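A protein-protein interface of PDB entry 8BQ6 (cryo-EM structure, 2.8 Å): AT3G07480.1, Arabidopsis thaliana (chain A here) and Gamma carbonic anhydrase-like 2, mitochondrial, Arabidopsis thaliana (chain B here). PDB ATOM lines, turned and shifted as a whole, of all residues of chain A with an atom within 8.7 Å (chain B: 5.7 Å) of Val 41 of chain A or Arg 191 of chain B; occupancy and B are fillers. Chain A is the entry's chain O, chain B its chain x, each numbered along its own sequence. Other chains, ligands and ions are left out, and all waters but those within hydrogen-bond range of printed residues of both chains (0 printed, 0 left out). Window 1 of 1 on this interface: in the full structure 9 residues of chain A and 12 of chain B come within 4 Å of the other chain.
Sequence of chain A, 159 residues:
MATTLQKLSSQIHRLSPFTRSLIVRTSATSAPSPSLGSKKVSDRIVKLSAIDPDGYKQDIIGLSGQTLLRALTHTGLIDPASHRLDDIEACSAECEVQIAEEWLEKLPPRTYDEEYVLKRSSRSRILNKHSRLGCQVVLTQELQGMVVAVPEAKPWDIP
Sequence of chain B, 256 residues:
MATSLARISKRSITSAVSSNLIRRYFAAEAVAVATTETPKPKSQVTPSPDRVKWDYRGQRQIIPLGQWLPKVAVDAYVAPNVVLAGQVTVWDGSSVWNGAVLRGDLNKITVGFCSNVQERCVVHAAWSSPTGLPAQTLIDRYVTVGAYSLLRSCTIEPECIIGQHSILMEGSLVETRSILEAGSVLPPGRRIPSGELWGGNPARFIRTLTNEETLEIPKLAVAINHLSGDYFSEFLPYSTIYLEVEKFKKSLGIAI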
ATOM      1  N   GLY A  37      -5.367   5.474  28.571  1.00  0.00           N
ATOM      2  CA  GLY A  37      -6.105   4.646  29.508  1.00  0.00           C
ATOM      3  C   GLY A  37      -5.701   4.895  30.941  1.00  0.00           C
ATOM      4  O   GLY A  37      -5.678   3.975  31.760  1.00  0.00           O
ATOM      5  N   SER A  38      -5.330   6.147  31.213  1.00  0.00           N
ATOM      6  CA  SER A  38      -4.956   6.629  32.535  1.00  0.00           C
ATOM      7  C   SER A  38      -3.609   6.061  32.961  1.00  0.00           C
ATOM      8  O   SER A  38      -3.028   6.548  33.929  1.00  0.00           O
ATOM      9  CB  SER A  38      -6.044   6.296  33.566  1.00  0.00           C
ATOM     10  OG  SER A  38      -5.665   6.675  34.878  1.00  0.00           O
ATOM     11  N   LYS A  39      -3.079   5.100  32.200  1.00  0.00           N
ATOM     12  CA  LYS A  39      -1.806   4.442  32.500  1.00  0.00           C
ATOM     13  C   LYS A  39      -1.166   4.056  31.174  1.00  0.00           C
ATOM     14  O   LYS A  39      -1.524   3.034  30.584  1.00  0.00           O
ATOM     15  CB  LYS A  39      -2.003   3.208  33.378  1.00  0.00           C
ATOM     16  CG  LYS A  39      -2.627   3.430  34.760  1.00  0.00           C
ATOM     17  CD  LYS A  39      -1.795   4.272  35.688  1.00  0.00           C
ATOM     18  CE  LYS A  39      -2.397   4.415  37.062  1.00  0.00           C
ATOM     19  NZ  LYS A  39      -1.560   5.272  37.944  1.00  0.00           N
ATOM     20  N   LYS A  40      -0.220   4.861  30.713  1.00  0.00           N
ATOM     21  CA  LYS A  40       0.417   4.643  29.429  1.00  0.00           C
ATOM     22  C   LYS A  40       1.865   4.226  29.635  1.00  0.00           C
ATOM     23  O   LYS A  40       2.464   4.477  30.683  1.00  0.00           O
ATOM     24  CB  LYS A  40       0.347   5.901  28.568  1.00  0.00           C
ATOM     25  CG  LYS A  40      -1.064   6.371  28.297  1.00  0.00           C
ATOM     26  CD  LYS A  40      -1.032   7.595  27.418  1.00  0.00           C
ATOM     27  CE  LYS A  40      -2.217   7.646  26.479  1.00  0.00           C
ATOM     28  NZ  LYS A  40      -3.477   7.980  27.185  1.00  0.00           N
ATOM     29  N   VAL A  41       2.424   3.564  28.622  1.00  0.00           N
ATOM     30  CA  VAL A  41       3.848   3.264  28.678  1.00  0.00           C
ATOM     31  C   VAL A  41       4.656   4.546  28.547  1.00  0.00           C
ATOM     32  O   VAL A  41       5.837   4.584  28.911  1.00  0.00           O
ATOM     33  CB  VAL A  41       4.235   2.237  27.600  1.00  0.00           C
ATOM     34  CG1 VAL A  41       3.263   1.073  27.600  1.00  0.00           C
ATOM     35  CG2 VAL A  41       4.271   2.896  26.258  1.00  0.00           C
ATOM     36  N   SER A  42       4.037   5.617  28.040  1.00  0.00           N
ATOM     37  CA  SER A  42       4.722   6.903  27.969  1.00  0.00           C
ATOM     38  C   SER A  42       4.989   7.479  29.352  1.00  0.00           C
ATOM     39  O   SER A  42       5.849   8.354  29.503  1.00  0.00           O
ATOM     40  CB  SER A  42       3.908   7.888  27.133  1.00  0.00           C
ATOM     41  OG  SER A  42       4.258   7.791  25.765  1.00  0.00           O
ATOM     42  N   ASP A  43       4.264   7.013  30.370  1.00  0.00           N
ATOM     43  CA  ASP A  43       4.557   7.431  31.736  1.00  0.00           C
ATOM     44  C   ASP A  43       5.905   6.923  32.211  1.00  0.00           C
ATOM     45  O   ASP A  43       6.505   7.524  33.108  1.00  0.00           O
ATOM     46  CB  ASP A  43       3.472   6.934  32.685  1.00  0.00           C
ATOM     47  CG  ASP A  43       2.091   7.329  32.237  1.00  0.00           C
ATOM     48  OD1 ASP A  43       1.128   6.604  32.558  1.00  0.00           O
ATOM     49  OD2 ASP A  43       1.970   8.367  31.558  1.00  0.00           O
ATOM     50  N   ARG A  44       6.383   5.822  31.642  1.00  0.00           N
ATOM     51  CA  ARG A  44       7.639   5.222  32.048  1.00  0.00           C
ATOM     52  C   ARG A  44       8.770   5.508  31.080  1.00  0.00           C
ATOM     53  O   ARG A  44       9.927   5.227  31.408  1.00  0.00           O
ATOM     54  CB  ARG A  44       7.466   3.707  32.197  1.00  0.00           C
ATOM     55  CG  ARG A  44       6.752   3.326  33.461  1.00  0.00           C
ATOM     56  CD  ARG A  44       6.616   1.838  33.568  1.00  0.00           C
ATOM     57  NE  ARG A  44       7.918   1.195  33.667  1.00  0.00           N
ATOM     58  CZ  ARG A  44       8.109  -0.111  33.560  1.00  0.00           C
ATOM     59  NH1 ARG A  44       7.099  -0.943  33.369  1.00  0.00           N
ATOM     60  NH2 ARG A  44       9.344  -0.594  33.652  1.00  0.00           N
ATOM     61  N   ILE A  45       8.463   6.059  29.908  1.00  0.00           N
ATOM     62  CA  ILE A  45       9.480   6.352  28.912  1.00  0.00           C
ATOM     63  C   ILE A  45      10.457   7.388  29.451  1.00  0.00           C
ATOM     64  O   ILE A  45      10.070   8.335  30.147  1.00  0.00           O
ATOM     65  CB  ILE A  45       8.815   6.817  27.606  1.00  0.00           C
ATOM     66  CG1 ILE A  45       8.222   5.618  26.870  1.00  0.00           C
ATOM     67  CG2 ILE A  45       9.781   7.588  26.731  1.00  0.00           C
ATOM     68  CD1 ILE A  45       7.794   5.925  25.474  1.00  0.00           C
ATOM     69  N   VAL A  46      11.738   7.179  29.160  1.00  0.00           N
ATOM     70  CA  VAL A  46      12.810   8.099  29.514  1.00  0.00           C
ATOM     71  C   VAL A  46      13.562   8.430  28.233  1.00  0.00           C
ATOM     72  O   VAL A  46      14.061   7.524  27.554  1.00  0.00           O
ATOM     73  CB  VAL A  46      13.756   7.494  30.562  1.00  0.00           C
ATOM     74  CG1 VAL A  46      14.867   8.466  30.899  1.00  0.00           C
ATOM     75  CG2 VAL A  46      12.984   7.089  31.808  1.00  0.00           C
ATOM     76  N   ILE A  61      15.502   5.475  23.480  1.00  0.00           N
ATOM     77  CA  ILE A  61      14.302   5.446  24.299  1.00  0.00           C
ATOM     78  C   ILE A  61      14.393   4.274  25.268  1.00  0.00           C
ATOM     79  O   ILE A  61      14.905   3.205  24.920  1.00  0.00           O
ATOM     80  CB  ILE A  61      13.038   5.373  23.412  1.00  0.00           C
ATOM     81  CG1 ILE A  61      11.923   6.184  24.045  1.00  0.00           C
ATOM     82  CG2 ILE A  61      12.596   3.953  23.147  1.00  0.00           C
ATOM     83  CD1 ILE A  61      12.335   7.594  24.256  1.00  0.00           C
ATOM     84  N   GLY A  62      13.936   4.492  26.499  1.00  0.00           N
ATOM     85  CA  GLY A  62      13.950   3.444  27.504  1.00  0.00           C
ATOM     86  C   GLY A  62      12.835   3.634  28.509  1.00  0.00           C
ATOM     87  O   GLY A  62      12.211   4.695  28.583  1.00  0.00           O
ATOM     88  N   LEU A  63      12.596   2.585  29.292  1.00  0.00           N
ATOM     89  CA  LEU A  63      11.573   2.600  30.328  1.00  0.00           C
ATOM     90  C   LEU A  63      12.214   2.798  31.696  1.00  0.00           C
ATOM     91  O   LEU A  63      13.216   2.155  32.018  1.00  0.00           O
ATOM     92  CB  LEU A  63      10.787   1.289  30.329  1.00  0.00           C
ATOM     93  CG  LEU A  63       9.823   0.996  29.183  1.00  0.00           C
ATOM     94  CD1 LEU A  63       8.991  -0.233  29.509  1.00  0.00           C
ATOM     95  CD2 LEU A  63       8.938   2.192  28.894  1.00  0.00           C
ATOM     96  N   SER A  64      11.624   3.676  32.505  1.00  0.00           N
ATOM     97  CA  SER A  64      12.091   3.822  33.878  1.00  0.00           C
ATOM     98  C   SER A  64      11.879   2.516  34.629  1.00  0.00           C
ATOM     99  O   SER A  64      10.937   1.768  34.355  1.00  0.00           O
ATOM    100  CB  SER A  64      11.359   4.958  34.590  1.00  0.00           C
ATOM    101  OG  SER A  64       9.963   4.726  34.631  1.00  0.00           O
ATOM    102  N   GLN A 141      13.061   8.973  36.103  1.00  0.00           N
ATOM    103  CA  GLN A 141      12.597  10.186  35.442  1.00  0.00           C
ATOM    104  C   GLN A 141      13.587  11.332  35.607  1.00  0.00           C
ATOM    105  O   GLN A 141      13.631  12.231  34.763  1.00  0.00           O
ATOM    106  CB  GLN A 141      11.223  10.587  35.977  1.00  0.00           C
ATOM    107  CG  GLN A 141      10.082   9.720  35.473  1.00  0.00           C
ATOM    108  CD  GLN A 141       9.991   9.677  33.962  1.00  0.00           C
ATOM    109  OE1 GLN A 141      10.353  10.630  33.275  1.00  0.00           O
ATOM    110  NE2 GLN A 141       9.512   8.559  33.435  1.00  0.00           N
ATOM    111  N   THR B 131       4.618   3.782  20.629  1.00  0.00           N
ATOM    112  CA  THR B 131       5.440   4.138  21.777  1.00  0.00           C
ATOM    113  C   THR B 131       6.910   4.303  21.424  1.00  0.00           C
ATOM    114  O   THR B 131       7.674   4.806  22.254  1.00  0.00           O
ATOM    115  CB  THR B 131       5.290   3.079  22.864  1.00  0.00           C
ATOM    116  OG1 THR B 131       6.209   2.007  22.619  1.00  0.00           O
ATOM    117  CG2 THR B 131       3.881   2.534  22.869  1.00  0.00           C
ATOM    118  N   LEU B 133       9.051   1.887  21.030  1.00  0.00           N
ATOM    119  CA  LEU B 133       9.835   0.752  21.466  1.00  0.00           C
ATOM    120  C   LEU B 133       9.809  -0.335  20.388  1.00  0.00           C
ATOM    121  O   LEU B 133       9.028  -0.254  19.439  1.00  0.00           O
ATOM    122  CB  LEU B 133       9.292   0.234  22.793  1.00  0.00           C
ATOM    123  CG  LEU B 133       9.589   1.102  24.018  1.00  0.00           C
ATOM    124  CD1 LEU B 133       8.731   0.635  25.159  1.00  0.00           C
ATOM    125  CD2 LEU B 133      11.053   1.062  24.411  1.00  0.00           C
ATOM    126  N   GLY B 171       2.010  -1.801  20.947  1.00  0.00           N
ATOM    127  CA  GLY B 171       2.827  -1.137  21.933  1.00  0.00           C
ATOM    128  C   GLY B 171       2.307  -1.206  23.349  1.00  0.00           C
ATOM    129  O   GLY B 171       2.926  -0.618  24.243  1.00  0.00           O
ATOM    130  N   SER B 172       1.194  -1.894  23.584  1.00  0.00           N
ATOM    131  CA  SER B 172       0.661  -1.983  24.931  1.00  0.00           C
ATOM    132  C   SER B 172       1.524  -2.913  25.775  1.00  0.00           C
ATOM    133  O   SER B 172       2.206  -3.808  25.269  1.00  0.00           O
ATOM    134  CB  SER B 172      -0.788  -2.466  24.908  1.00  0.00           C
ATOM    135  OG  SER B 172      -0.899  -3.718  24.258  1.00  0.00           O
ATOM    136  N   LEU B 173       1.506  -2.679  27.080  1.00  0.00           N
ATOM    137  CA  LEU B 173       2.378  -3.410  27.982  1.00  0.00           C
ATOM    138  C   LEU B 173       1.577  -3.885  29.180  1.00  0.00           C
ATOM    139  O   LEU B 173       0.874  -3.095  29.812  1.00  0.00           O
ATOM    140  CB  LEU B 173       3.548  -2.535  28.432  1.00  0.00           C
ATOM    141  CG  LEU B 173       4.399  -3.034  29.595  1.00  0.00           C
ATOM    142  CD1 LEU B 173       5.170  -4.291  29.214  1.00  0.00           C
ATOM    143  CD2 LEU B 173       5.342  -1.935  30.025  1.00  0.00           C
ATOM    144  N   VAL B 174       1.683  -5.171  29.481  1.00  0.00           N
ATOM    145  CA  VAL B 174       1.091  -5.744  30.678  1.00  0.00           C
ATOM    146  C   VAL B 174       2.244  -6.125  31.588  1.00  0.00           C
ATOM    147  O   VAL B 174       3.053  -6.993  31.242  1.00  0.00           O
ATOM    148  CB  VAL B 174       0.208  -6.956  30.359  1.00  0.00           C
ATOM    149  CG1 VAL B 174      -0.507  -7.424  31.612  1.00  0.00           C
ATOM    150  CG2 VAL B 174      -0.780  -6.619  29.254  1.00  0.00           C
ATOM    151  N   GLU B 175       2.334  -5.473  32.742  1.00  0.00           N
ATOM    152  CA  GLU B 175       3.432  -5.738  33.652  1.00  0.00           C
ATOM    153  C   GLU B 175       3.177  -7.021  34.433  1.00  0.00           C
ATOM    154  O   GLU B 175       2.055  -7.529  34.501  1.00  0.00           O
ATOM    155  CB  GLU B 175       3.640  -4.565  34.603  1.00  0.00           C
ATOM    156  CG  GLU B 175       3.947  -3.275  33.892  1.00  0.00           C
ATOM    157  CD  GLU B 175       4.207  -2.141  34.850  1.00  0.00           C
ATOM    158  OE1 GLU B 175       4.250  -2.385  36.072  1.00  0.00           O
ATOM    159  OE2 GLU B 175       4.357  -0.998  34.383  1.00  0.00           O
ATOM    160  N   LEU B 186      -7.313  -3.212  25.553  1.00  0.00           N
ATOM    161  CA  LEU B 186      -6.200  -2.338  25.894  1.00  0.00           C
ATOM    162  C   LEU B 186      -5.765  -1.551  24.667  1.00  0.00           C
ATOM    163  O   LEU B 186      -5.160  -2.133  23.755  1.00  0.00           O
ATOM    164  CB  LEU B 186      -5.031  -3.150  26.445  1.00  0.00           C
ATOM    165  CG  LEU B 186      -3.968  -2.376  27.227  1.00  0.00           C
ATOM    166  CD1 LEU B 186      -4.597  -1.623  28.376  1.00  0.00           C
ATOM    167  CD2 LEU B 186      -2.887  -3.305  27.739  1.00  0.00           C
ATOM    168  N   GLY B 189      -0.358   1.515  23.155  1.00  0.00           N
ATOM    169  CA  GLY B 189       0.528   2.235  24.040  1.00  0.00           C
ATOM    170  C   GLY B 189       0.104   2.284  25.487  1.00  0.00           C
ATOM    171  O   GLY B 189       0.759   2.968  26.281  1.00  0.00           O
ATOM    172  N   ARG B 190      -0.961   1.585  25.860  1.00  0.00           N
ATOM    173  CA  ARG B 190      -1.414   1.605  27.241  1.00  0.00           C
ATOM    174  C   ARG B 190      -0.647   0.582  28.062  1.00  0.00           C
ATOM    175  O   ARG B 190       0.054  -0.282  27.535  1.00  0.00           O
ATOM    176  CB  ARG B 190      -2.911   1.328  27.334  1.00  0.00           C
ATOM    177  CG  ARG B 190      -3.770   2.568  27.301  1.00  0.00           C
ATOM    178  CD  ARG B 190      -3.552   3.329  26.017  1.00  0.00           C
ATOM    179  NE  ARG B 190      -4.542   4.380  25.839  1.00  0.00           N
ATOM    180  CZ  ARG B 190      -4.748   5.028  24.703  1.00  0.00           C
ATOM    181  NH1 ARG B 190      -4.012   4.794  23.629  1.00  0.00           N
ATOM    182  NH2 ARG B 190      -5.724   5.927  24.640  1.00  0.00           N
ATOM    183  N   ARG B 191      -0.797   0.684  29.375  1.00  0.00           N
ATOM    184  CA  ARG B 191       0.002  -0.093  30.304  1.00  0.00           C
ATOM    185  C   ARG B 191      -0.873  -0.617  31.430  1.00  0.00           C
ATOM    186  O   ARG B 191      -1.736   0.100  31.943  1.00  0.00           O
ATOM    187  CB  ARG B 191       1.146   0.767  30.853  1.00  0.00           C
ATOM    188  CG  ARG B 191       1.828   0.216  32.075  1.00  0.00           C
ATOM    189  CD  ARG B 191       3.067   1.024  32.393  1.00  0.00           C
ATOM    190  NE  ARG B 191       2.752   2.360  32.877  1.00  0.00           N
ATOM    191  CZ  ARG B 191       2.582   2.664  34.155  1.00  0.00           C
ATOM    192  NH1 ARG B 191       2.659   1.741  35.100  1.00  0.00           N
ATOM    193  NH2 ARG B 191       2.327   3.923  34.494  1.00  0.00           N
ATOM    194  N   ILE B 192      -0.661  -1.874  31.804  1.00  0.00           N
ATOM    195  CA  ILE B 192      -1.290  -2.455  32.983  1.00  0.00           C
ATOM    196  C   ILE B 192      -0.215  -2.579  34.060  1.00  0.00           C
ATOM    197  O   ILE B 192       0.698  -3.408  33.928  1.00  0.00           O
ATOM    198  CB  ILE B 192      -1.931  -3.815  32.684  1.00  0.00           C
ATOM    199  CG1 ILE B 192      -2.883  -3.715  31.492  1.00  0.00           C
ATOM    200  CG2 ILE B 192      -2.667  -4.318  33.908  1.00  0.00           C
ATOM    201  CD1 ILE B 192      -4.130  -2.920  31.768  1.00  0.00           C
ATOM    202  N   PRO B 193      -0.270  -1.787  35.125  1.00  0.00           N
ATOM    203  CA  PRO B 193       0.786  -1.841  36.137  1.00  0.00           C
ATOM    204  C   PRO B 193       0.767  -3.153  36.901  1.00  0.00           C
ATOM    205  O   PRO B 193      -0.258  -3.828  37.009  1.00  0.00           O
ATOM    206  CB  PRO B 193       0.473  -0.652  37.056  1.00  0.00           C
ATOM    207  CG  PRO B 193      -0.638   0.104  36.392  1.00  0.00           C
ATOM    208  CD  PRO B 193      -1.338  -0.846  35.490  1.00  0.00           C
ATOM    209  N   TRP B 198      -7.369  -5.511  36.024  1.00  0.00           N
ATOM    210  CA  TRP B 198      -7.969  -4.522  35.144  1.00  0.00           C
ATOM    211  C   TRP B 198      -9.044  -5.198  34.308  1.00  0.00           C
ATOM    212  O   TRP B 198      -9.113  -6.426  34.230  1.00  0.00           O
ATOM    213  CB  TRP B 198      -6.921  -3.875  34.233  1.00  0.00           C
ATOM    214  CG  TRP B 198      -6.081  -2.839  34.901  1.00  0.00           C
ATOM    215  CD1 TRP B 198      -5.309  -2.997  36.010  1.00  0.00           C
ATOM    216  CD2 TRP B 198      -5.910  -1.484  34.483  1.00  0.00           C
ATOM    217  NE1 TRP B 198      -4.675  -1.820  36.317  1.00  0.00           N
ATOM    218  CE2 TRP B 198      -5.029  -0.875  35.392  1.00  0.00           C
ATOM    219  CE3 TRP B 198      -6.423  -0.725  33.432  1.00  0.00           C
ATOM    220  CZ2 TRP B 198      -4.649   0.455  35.281  1.00  0.00           C
ATOM    221  CZ3 TRP B 198      -6.049   0.593  33.326  1.00  0.00           C
ATOM    222  CH2 TRP B 198      -5.169   1.170  34.243  1.00  0.00           C
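The backbone carbonyl oxygen of Lys 39 of chain A is in hydrogen-bond range of the backbone NH of Arg 191 of chain B, at 2.7 Å. The backbone carbonyl oxygen of Lys 40 of chain A sits at hydrogen-bond distance from the guanidinium group of Arg 191 of chain B (3.1 Å). The backbone NH of Val 41 of chain A sits at hydrogen-bond distance from the backbone carbonyl oxygen of Gly 189 of chain B, at 2.9 Å. The side-chain carboxylate (OD1) of Asp 43 of chain A lies within salt-bridge range of the guanidinium group (NH2) of Arg 191 of chain B (3.5 Å). NH1 of Arg 44 of chain A is in salt-bridge range of OE2 of Glu 175 of chain B, at 2.9 Å. N of Gly 37 of chain A lies close to NE of Arg 190 of chain B, 3.1 Å away.
OD1 of Asp 43 of chain A lies within hydrogen-bond range of N of Lys 40 of chain A, 2.9 Å away. The backbone carbonyl oxygen (O) of Asp 43 of chain A sits at hydrogen-bond distance from the side-chain amide nitrogen (NE2) of Gln 141 of chain A, 3.2 Å away. O of Arg 44 of chain A is in hydrogen-bond range of N of Ser 64 of chain A. NE2 of Gln 141 of chain A sits at hydrogen-bond distance from O of Ile 45 of chain A, at 3.3 Å. The backbone carbonyl oxygen (O) of Leu 173 of chain B lies within hydrogen-bond range of the backbone NH (N) of Ile 192 of chain B (2.8 Å). The backbone NH (N) of Glu 175 of chain B lies within hydrogen-bond range of the backbone carbonyl oxygen (O) of Ile 192 of chain B (2.9 Å).
O of Gly 37 of chain A touches CZ3 of Trp 198 of chain B, at 3.7 Å. Lys 39 of chain A touches Arg 190 of chain B. Lys 39 of chain A touches Trp 198 of chain B. Gly 189 of chain B touches Lys 40 of chain A (O to CA, 3.6 Å). Arg 190 of chain B touches Lys 40 of chain A. Val 41 of chain A touches Thr 131 of chain B. Val 41 of chain A touches Arg 191 of chain B. NH1 of Arg 44 of chain A touches CD2 of Leu 173 of chain B (3.9 Å). CD of Arg 44 of chain A touches CD of Arg 191 of chain B (3.8 Å). Leu 133 of chain B touches Ile 61 of chain A.
Of the printed residues of chain B, Lys 40 of chain A touches Gly 189, Arg 190 and Arg 191. Val 41 of chain A touches six residues of chain B. Printed residues of chain B within 4 Å of Ile 61 of chain A: Leu 133. Gln 141 of chain A touches none of the printed residues of chain B. Of the printed residues of chain A, Gly 189 of chain B touches Lys 40 (3.6 Å) and Val 41 (2.9 Å). Of the printed residues of chain A, Arg 190 of chain B touches Gly 37 (3.1 Å), Lys 39 (3.6 Å), Lys 40 (3.97 Å) and Val 41 (3.5 Å). Arg 191 of chain B touches just these residues of chain A: Lys 39, Lys 40, Val 41, Asp 43 and Arg 44. The nearest printed residue of chain B that does not touch Lys 39 of chain A is Pro 193 of chain B (4.2 Å).
Of the 14 printed residues of chain B, 9 touch a printed residue of chain A. Hydrophobic or aromatic side chains of chain A within 4 Å of the printed part of chain B: Val 41, Ile 45 and Ile 61. Among the printed residues, 20 pairs touch across the chains. Among the printed residues, Asp or Glu carboxylates within 4 Å of a Lys or Arg side-chain nitrogen of the other chain: Asp 43 of chain A with Arg 191 of chain B and Arg 44 of chain A with Glu 175 of chain B.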
